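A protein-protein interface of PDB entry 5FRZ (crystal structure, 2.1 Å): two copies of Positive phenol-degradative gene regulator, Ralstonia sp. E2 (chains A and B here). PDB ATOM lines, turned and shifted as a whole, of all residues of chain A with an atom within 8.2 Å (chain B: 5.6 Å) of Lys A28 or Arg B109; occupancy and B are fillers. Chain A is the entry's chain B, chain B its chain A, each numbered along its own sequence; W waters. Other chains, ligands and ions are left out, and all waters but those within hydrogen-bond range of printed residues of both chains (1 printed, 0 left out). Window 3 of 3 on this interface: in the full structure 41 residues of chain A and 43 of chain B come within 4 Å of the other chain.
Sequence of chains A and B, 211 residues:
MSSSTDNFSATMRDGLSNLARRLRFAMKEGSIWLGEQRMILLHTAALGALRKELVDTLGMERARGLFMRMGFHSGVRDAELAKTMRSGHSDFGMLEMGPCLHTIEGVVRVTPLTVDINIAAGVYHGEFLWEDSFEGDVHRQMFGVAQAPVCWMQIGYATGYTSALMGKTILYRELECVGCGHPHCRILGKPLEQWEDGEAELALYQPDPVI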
ATOM      1  N   ARG A  24     -33.586  30.318 -16.321  1.00  0.00           N
ATOM      2  CA  ARG A  24     -32.276  29.745 -16.019  1.00  0.00           C
ATOM      3  C   ARG A  24     -31.584  29.108 -17.236  1.00  0.00           C
ATOM      4  O   ARG A  24     -32.221  28.482 -18.095  1.00  0.00           O
ATOM      5  CB  ARG A  24     -32.409  28.724 -14.889  1.00  0.00           C
ATOM      6  CG  ARG A  24     -33.284  27.542 -15.227  1.00  0.00           C
ATOM      7  CD  ARG A  24     -33.577  26.695 -13.997  1.00  0.00           C
ATOM      8  NE  ARG A  24     -34.476  25.595 -14.321  1.00  0.00           N
ATOM      9  CZ  ARG A  24     -34.060  24.437 -14.820  1.00  0.00           C
ATOM     10  NH1 ARG A  24     -32.762  24.252 -15.044  1.00  0.00           N
ATOM     11  NH2 ARG A  24     -34.928  23.470 -15.103  1.00  0.00           N
ATOM     12  N   PHE A  25     -30.274  29.299 -17.302  1.00  0.00           N
ATOM     13  CA  PHE A  25     -29.441  28.713 -18.350  1.00  0.00           C
ATOM     14  C   PHE A  25     -28.807  27.421 -17.863  1.00  0.00           C
ATOM     15  O   PHE A  25     -28.036  27.435 -16.909  1.00  0.00           O
ATOM     16  CB  PHE A  25     -28.341  29.690 -18.790  1.00  0.00           C
ATOM     17  CG  PHE A  25     -28.823  30.788 -19.698  1.00  0.00           C
ATOM     18  CD1 PHE A  25     -29.655  31.796 -19.216  1.00  0.00           C
ATOM     19  CD2 PHE A  25     -28.442  30.817 -21.035  1.00  0.00           C
ATOM     20  CE1 PHE A  25     -30.103  32.808 -20.050  1.00  0.00           C
ATOM     21  CE2 PHE A  25     -28.884  31.839 -21.880  1.00  0.00           C
ATOM     22  CZ  PHE A  25     -29.719  32.831 -21.382  1.00  0.00           C
ATOM     23  N   ALA A  26     -29.131  26.308 -18.517  1.00  0.00           N
ATOM     24  CA  ALA A  26     -28.550  25.016 -18.165  1.00  0.00           C
ATOM     25  C   ALA A  26     -27.627  24.529 -19.272  1.00  0.00           C
ATOM     26  O   ALA A  26     -28.011  23.670 -20.066  1.00  0.00           O
ATOM     27  CB  ALA A  26     -29.650  23.992 -17.904  1.00  0.00           C
ATOM     28  N   MET A  27     -26.420  25.077 -19.328  1.00  0.00           N
ATOM     29  CA  MET A  27     -25.533  24.777 -20.443  1.00  0.00           C
ATOM     30  C   MET A  27     -25.179  23.294 -20.469  1.00  0.00           C
ATOM     31  O   MET A  27     -24.889  22.761 -21.527  1.00  0.00           O
ATOM     32  CB  MET A  27     -24.258  25.627 -20.392  1.00  0.00           C
ATOM     33  CG  MET A  27     -23.854  26.054 -18.998  1.00  0.00           C
ATOM     34  SD  MET A  27     -22.648  27.396 -19.154  1.00  0.00           S
ATOM     35  CE  MET A  27     -23.402  28.381 -20.447  1.00  0.00           C
ATOM     36  N   LYS A  28     -25.189  22.629 -19.322  1.00  0.00           N
ATOM     37  CA  LYS A  28     -24.740  21.258 -19.275  1.00  0.00           C
ATOM     38  C   LYS A  28     -25.772  20.378 -20.011  1.00  0.00           C
ATOM     39  O   LYS A  28     -25.511  19.227 -20.401  1.00  0.00           O
ATOM     40  CB  LYS A  28     -24.490  20.873 -17.805  1.00  0.00           C
ATOM     41  CG  LYS A  28     -25.551  21.142 -16.826  1.00  0.00           C
ATOM     42  CD  LYS A  28     -25.618  19.989 -15.732  1.00  0.00           C
ATOM     43  CE  LYS A  28     -27.001  19.920 -14.993  1.00  0.00           C
ATOM     44  NZ  LYS A  28     -27.572  21.083 -14.381  1.00  0.00           N
ATOM     45  N   GLU A  29     -26.995  20.901 -20.132  1.00  0.00           N
ATOM     46  CA  GLU A  29     -28.007  20.296 -21.042  1.00  0.00           C
ATOM     47  C   GLU A  29     -28.095  20.983 -22.397  1.00  0.00           C
ATOM     48  O   GLU A  29     -28.956  20.614 -23.205  1.00  0.00           O
ATOM     49  CB  GLU A  29     -29.451  20.295 -20.440  1.00  0.00           C
ATOM     50  CG  GLU A  29     -29.666  19.328 -19.249  1.00  0.00           C
ATOM     51  CD  GLU A  29     -29.190  19.937 -18.006  1.00  0.00           C
ATOM     52  OE1 GLU A  29     -28.013  19.859 -17.666  1.00  0.00           O
ATOM     53  OE2 GLU A  29     -30.028  20.570 -17.377  1.00  0.00           O
ATOM     54  N   GLY A  30     -27.279  22.026 -22.588  1.00  0.00           N
ATOM     55  CA  GLY A  30     -27.442  22.982 -23.675  1.00  0.00           C
ATOM     56  C   GLY A  30     -28.891  23.410 -23.754  1.00  0.00           C
ATOM     57  O   GLY A  30     -29.513  23.319 -24.807  1.00  0.00           O
ATOM     58  N   SER A  31     -29.461  23.829 -22.631  1.00  0.00           N
ATOM     59  CA  SER A  31     -30.871  24.196 -22.656  1.00  0.00           C
ATOM     60  C   SER A  31     -31.090  25.443 -21.820  1.00  0.00           C
ATOM     61  O   SER A  31     -30.239  25.829 -21.015  1.00  0.00           O
ATOM     62  CB  SER A  31     -31.751  23.031 -22.172  1.00  0.00           C
ATOM     63  OG  SER A  31     -31.389  22.616 -20.874  1.00  0.00           O
ATOM     64  N   TRP A  33     -34.320  27.443 -19.647  1.00  0.00           N
ATOM     65  CA  TRP A  33     -35.659  27.205 -19.102  1.00  0.00           C
ATOM     66  C   TRP A  33     -36.289  28.482 -18.555  1.00  0.00           C
ATOM     67  O   TRP A  33     -35.635  29.267 -17.865  1.00  0.00           O
ATOM     68  CB  TRP A  33     -35.599  26.129 -18.002  1.00  0.00           C
ATOM     69  CG  TRP A  33     -35.130  24.819 -18.514  1.00  0.00           C
ATOM     70  CD1 TRP A  33     -33.838  24.384 -18.589  1.00  0.00           C
ATOM     71  CD2 TRP A  33     -35.940  23.772 -19.063  1.00  0.00           C
ATOM     72  NE1 TRP A  33     -33.793  23.127 -19.151  1.00  0.00           N
ATOM     73  CE2 TRP A  33     -35.070  22.730 -19.447  1.00  0.00           C
ATOM     74  CE3 TRP A  33     -37.314  23.616 -19.269  1.00  0.00           C
ATOM     75  CZ2 TRP A  33     -35.533  21.545 -20.010  1.00  0.00           C
ATOM     76  CZ3 TRP A  33     -37.770  22.445 -19.830  1.00  0.00           C
ATOM     77  CH2 TRP A  33     -36.882  21.421 -20.194  1.00  0.00           C
ATOM     78  N   ARG A  38     -39.016  25.020 -22.033  1.00  0.00           N
ATOM     79  CA  ARG A  38     -37.719  25.127 -22.689  1.00  0.00           C
ATOM     80  C   ARG A  38     -37.751  26.272 -23.708  1.00  0.00           C
ATOM     81  O   ARG A  38     -38.692  26.401 -24.480  1.00  0.00           O
ATOM     82  CB  ARG A  38     -37.335  23.798 -23.363  1.00  0.00           C
ATOM     83  CG  ARG A  38     -35.878  23.732 -23.703  1.00  0.00           C
ATOM     84  CD  ARG A  38     -35.469  22.459 -24.442  1.00  0.00           C
ATOM     85  NE  ARG A  38     -34.104  22.615 -24.925  1.00  0.00           N
ATOM     86  CZ  ARG A  38     -33.353  21.638 -25.427  1.00  0.00           C
ATOM     87  NH1 ARG A  38     -33.831  20.400 -25.522  1.00  0.00           N
ATOM     88  NH2 ARG A  38     -32.124  21.914 -25.841  1.00  0.00           N
ATOM     89  N   THR B 103     -24.893  26.215 -28.020  1.00  0.00           N
ATOM     90  CA  THR B 103     -25.187  25.760 -26.654  1.00  0.00           C
ATOM     91  C   THR B 103     -25.671  26.914 -25.754  1.00  0.00           C
ATOM     92  O   THR B 103     -26.589  26.745 -24.925  1.00  0.00           O
ATOM     93  CB  THR B 103     -23.935  25.067 -26.024  1.00  0.00           C
ATOM     94  OG1 THR B 103     -23.642  23.870 -26.750  1.00  0.00           O
ATOM     95  CG2 THR B 103     -24.180  24.707 -24.571  1.00  0.00           C
ATOM     96  N   VAL B 107     -30.038  25.574 -27.872  1.00  0.00           N
ATOM     97  CA  VAL B 107     -30.491  24.742 -28.982  1.00  0.00           C
ATOM     98  C   VAL B 107     -30.099  23.262 -28.794  1.00  0.00           C
ATOM     99  O   VAL B 107     -30.907  22.364 -29.011  1.00  0.00           O
ATOM    100  CB  VAL B 107     -29.923  25.306 -30.329  1.00  0.00           C
ATOM    101  CG1 VAL B 107     -30.077  24.292 -31.481  1.00  0.00           C
ATOM    102  CG2 VAL B 107     -30.597  26.653 -30.665  1.00  0.00           C
ATOM    103  N   VAL B 108     -28.873  23.023 -28.347  1.00  0.00           N
ATOM    104  CA  VAL B 108     -28.292  21.682 -28.332  1.00  0.00           C
ATOM    105  C   VAL B 108     -26.948  21.751 -27.616  1.00  0.00           C
ATOM    106  O   VAL B 108     -26.346  22.826 -27.529  1.00  0.00           O
ATOM    107  CB  VAL B 108     -28.102  21.126 -29.784  1.00  0.00           C
ATOM    108  CG1 VAL B 108     -27.040  21.934 -30.549  1.00  0.00           C
ATOM    109  CG2 VAL B 108     -27.740  19.639 -29.777  1.00  0.00           C
ATOM    110  N   ARG B 109     -26.480  20.622 -27.089  1.00  0.00           N
ATOM    111  CA  ARG B 109     -25.098  20.523 -26.643  1.00  0.00           C
ATOM    112  C   ARG B 109     -24.278  19.616 -27.557  1.00  0.00           C
ATOM    113  O   ARG B 109     -24.689  18.497 -27.889  1.00  0.00           O
ATOM    114  CB  ARG B 109     -25.013  20.011 -25.207  1.00  0.00           C
ATOM    115  CG  ARG B 109     -24.145  20.908 -24.338  1.00  0.00           C
ATOM    116  CD  ARG B 109     -23.687  20.199 -23.084  1.00  0.00           C
ATOM    117  NE  ARG B 109     -22.545  19.326 -23.325  1.00  0.00           N
ATOM    118  CZ  ARG B 109     -21.894  18.686 -22.360  1.00  0.00           C
ATOM    119  NH1 ARG B 109     -22.281  18.826 -21.097  1.00  0.00           N
ATOM    120  NH2 ARG B 109     -20.856  17.916 -22.651  1.00  0.00           N
ATOM    121  N   VAL B 110     -23.107  20.106 -27.926  1.00  0.00           N
ATOM    122  CA  VAL B 110     -22.278  19.485 -28.944  1.00  0.00           C
ATOM    123  C   VAL B 110     -21.072  18.816 -28.329  1.00  0.00           C
ATOM    124  O   VAL B 110     -20.453  19.358 -27.404  1.00  0.00           O
ATOM    125  CB  VAL B 110     -21.757  20.520 -29.974  1.00  0.00           C
ATOM    126  CG1 VAL B 110     -21.276  19.818 -31.229  1.00  0.00           C
ATOM    127  CG2 VAL B 110     -22.814  21.531 -30.310  1.00  0.00           C
ATOM    128  N   THR B 111     -20.728  17.650 -28.858  1.00  0.00           N
ATOM    129  CA  THR B 111     -19.444  17.030 -28.565  1.00  0.00           C
ATOM    130  C   THR B 111     -18.724  16.718 -29.876  1.00  0.00           C
ATOM    131  O   THR B 111     -19.226  15.960 -30.704  1.00  0.00           O
ATOM    132  CB  THR B 111     -19.601  15.736 -27.714  1.00  0.00           C
ATOM    133  OG1 THR B 111     -20.096  16.077 -26.411  1.00  0.00           O
ATOM    134  CG2 THR B 111     -18.267  15.028 -27.561  1.00  0.00           C
ATOM    135  N   LEU B 129     -21.357  15.013 -32.060  1.00  0.00           N
ATOM    136  CA  LEU B 129     -22.530  14.525 -31.334  1.00  0.00           C
ATOM    137  C   LEU B 129     -23.436  15.687 -30.932  1.00  0.00           C
ATOM    138  O   LEU B 129     -22.960  16.731 -30.503  1.00  0.00           O
ATOM    139  CB  LEU B 129     -22.116  13.750 -30.076  1.00  0.00           C
ATOM    140  CG  LEU B 129     -21.394  12.409 -30.239  1.00  0.00           C
ATOM    141  CD1 LEU B 129     -21.089  11.773 -28.874  1.00  0.00           C
ATOM    142  CD2 LEU B 129     -22.227  11.458 -31.077  1.00  0.00           C
ATOM    143  N   TRP B 130     -24.737  15.491 -31.076  1.00  0.00           N
ATOM    144  CA  TRP B 130     -25.730  16.417 -30.562  1.00  0.00           C
ATOM    145  C   TRP B 130     -26.508  15.734 -29.460  1.00  0.00           C
ATOM    146  O   TRP B 130     -27.127  14.687 -29.680  1.00  0.00           O
ATOM    147  CB  TRP B 130     -26.693  16.861 -31.650  1.00  0.00           C
ATOM    148  CG  TRP B 130     -26.231  18.044 -32.461  1.00  0.00           C
ATOM    149  CD1 TRP B 130     -25.229  18.924 -32.160  1.00  0.00           C
ATOM    150  CD2 TRP B 130     -26.773  18.461 -33.708  1.00  0.00           C
ATOM    151  NE1 TRP B 130     -25.117  19.874 -33.156  1.00  0.00           N
ATOM    152  CE2 TRP B 130     -26.061  19.608 -34.117  1.00  0.00           C
ATOM    153  CE3 TRP B 130     -27.801  17.978 -34.522  1.00  0.00           C
ATOM    154  CZ2 TRP B 130     -26.353  20.281 -35.299  1.00  0.00           C
ATOM    155  CZ3 TRP B 130     -28.082  18.651 -35.707  1.00  0.00           C
ATOM    156  CH2 TRP B 130     -27.358  19.780 -36.081  1.00  0.00           C
ATOM    157  N   GLU B 131     -26.474  16.329 -28.277  1.00  0.00           N
ATOM    158  CA  GLU B 131     -27.248  15.821 -27.159  1.00  0.00           C
ATOM    159  C   GLU B 131     -28.252  16.869 -26.712  1.00  0.00           C
ATOM    160  O   GLU B 131     -27.954  18.063 -26.721  1.00  0.00           O
ATOM    161  CB  GLU B 131     -26.322  15.419 -26.020  1.00  0.00           C
ATOM    162  CG  GLU B 131     -25.488  14.192 -26.364  1.00  0.00           C
ATOM    163  CD  GLU B 131     -24.543  13.794 -25.255  1.00  0.00           C
ATOM    164  OE1 GLU B 131     -24.995  13.104 -24.315  1.00  0.00           O
ATOM    165  OE2 GLU B 131     -23.349  14.168 -25.325  1.00  0.00           O
ATOM    166  N   ASP B 132     -29.450  16.411 -26.367  1.00  0.00           N
ATOM    167  CA  ASP B 132     -30.516  17.294 -25.897  1.00  0.00           C
ATOM    168  C   ASP B 132     -30.909  18.317 -26.958  1.00  0.00           C
ATOM    169  O   ASP B 132     -31.158  19.476 -26.633  1.00  0.00           O
ATOM    170  CB  ASP B 132     -30.096  18.012 -24.611  1.00  0.00           C
ATOM    171  CG  ASP B 132     -30.094  17.086 -23.402  1.00  0.00           C
ATOM    172  OD1 ASP B 132     -30.648  15.971 -23.508  1.00  0.00           O
ATOM    173  OD2 ASP B 132     -29.550  17.471 -22.347  1.00  0.00           O
ATOM    174  N   SER B 133     -30.956  17.870 -28.216  1.00  0.00           N
ATOM    175  CA  SER B 133     -31.475  18.665 -29.327  1.00  0.00           C
ATOM    176  C   SER B 133     -32.873  19.198 -29.028  1.00  0.00           C
ATOM    177  O   SER B 133     -33.803  18.415 -28.836  1.00  0.00           O
ATOM    178  CB  SER B 133     -31.520  17.834 -30.609  1.00  0.00           C
ATOM    179  OG  SER B 133     -30.218  17.547 -31.105  1.00  0.00           O
HETATM  180  O   HOH W   1     -27.562  26.752 -22.254  1.00  0.00           O
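The backbone carbonyl oxygen of Val B107 is in hydrogen-bond range of the guanidinium group of Arg A38. The backbone carbonyl oxygen (O) of Lys A28 is in hydrogen-bond range of the guanidinium group (NH1) of Arg B109 (3.3 Å). The backbone carbonyl oxygen of Asp B132 sits at hydrogen-bond distance from the guanidinium group of Arg A38, 2.7 Å away. The side-chain carboxylate (OD2) of Asp B132 lies close to the backbone carbonyl oxygen (O) of Glu A29, at 3.3 Å.
O of Val B108 is in hydrogen-bond range of OG1 of Thr B103. The backbone carbonyl oxygen (O) of Arg B109 lies within hydrogen-bond range of the backbone NH (N) of Glu B131 (2.8 Å). OE1 of Glu A29 is in salt-bridge range of NZ of Lys A28, 3.5 Å away. The backbone carbonyl oxygen (O) of Gly A30 lies within hydrogen-bond range of the guanidinium group (NH2) of Arg A38 (3.1 Å).
O of Met A27 touches CG2 of Thr B103 (3.7 Å). Met A27 touches Arg B109 (O to CD, 3.2 Å). CA of Gly A30 touches CG2 of Thr B103, 3.8 Å away. Gly A30 touches Val B107. O of Gly A30 touches N of Val B108, 3.6 Å away. Arg B109 touches Gly A30. Ser B133 touches Arg A38 (C to NH1, 3.8 Å).
Lys A28 touches just one residue of chain B: Arg B109. Of the printed residues of chain B, Glu A29 touches Asp B132 (3.2 Å). Of the printed residues of chain B, Gly A30 touches Thr B103 (3.8 Å), Val B107 (3.8 Å), Val B108 (3.6 Å) and Arg B109 (3.8 Å). Printed residues of chain B within 4 Å of Arg A38: Val B107, Asp B132 and Ser B133. Of the printed residues of chain A, Thr B103 touches Met A27 (3.7 Å) and Gly A30 (3.8 Å). Arg B109 touches just these residues of chain A: Met A27 (3.2 Å), Lys A28 (3.3 Å) and Gly A30 (3.8 Å).
Of the 10 printed residues of chain A, 5 touch a printed residue of chain B. Along chain A the printed residues that touch a printed residue of chain B span positions 27 to 38.
No position is printed for both chains. Of the 11 pairs that touch across the chains among the printed residues, none has its exchanged pair printed and touching as well.
Water W1 bridges the backbone carbonyl oxygen (O) of Thr B103 (2.8 Å) and the backbone carbonyl oxygen (O) of Ser A31 (3.1 Å).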
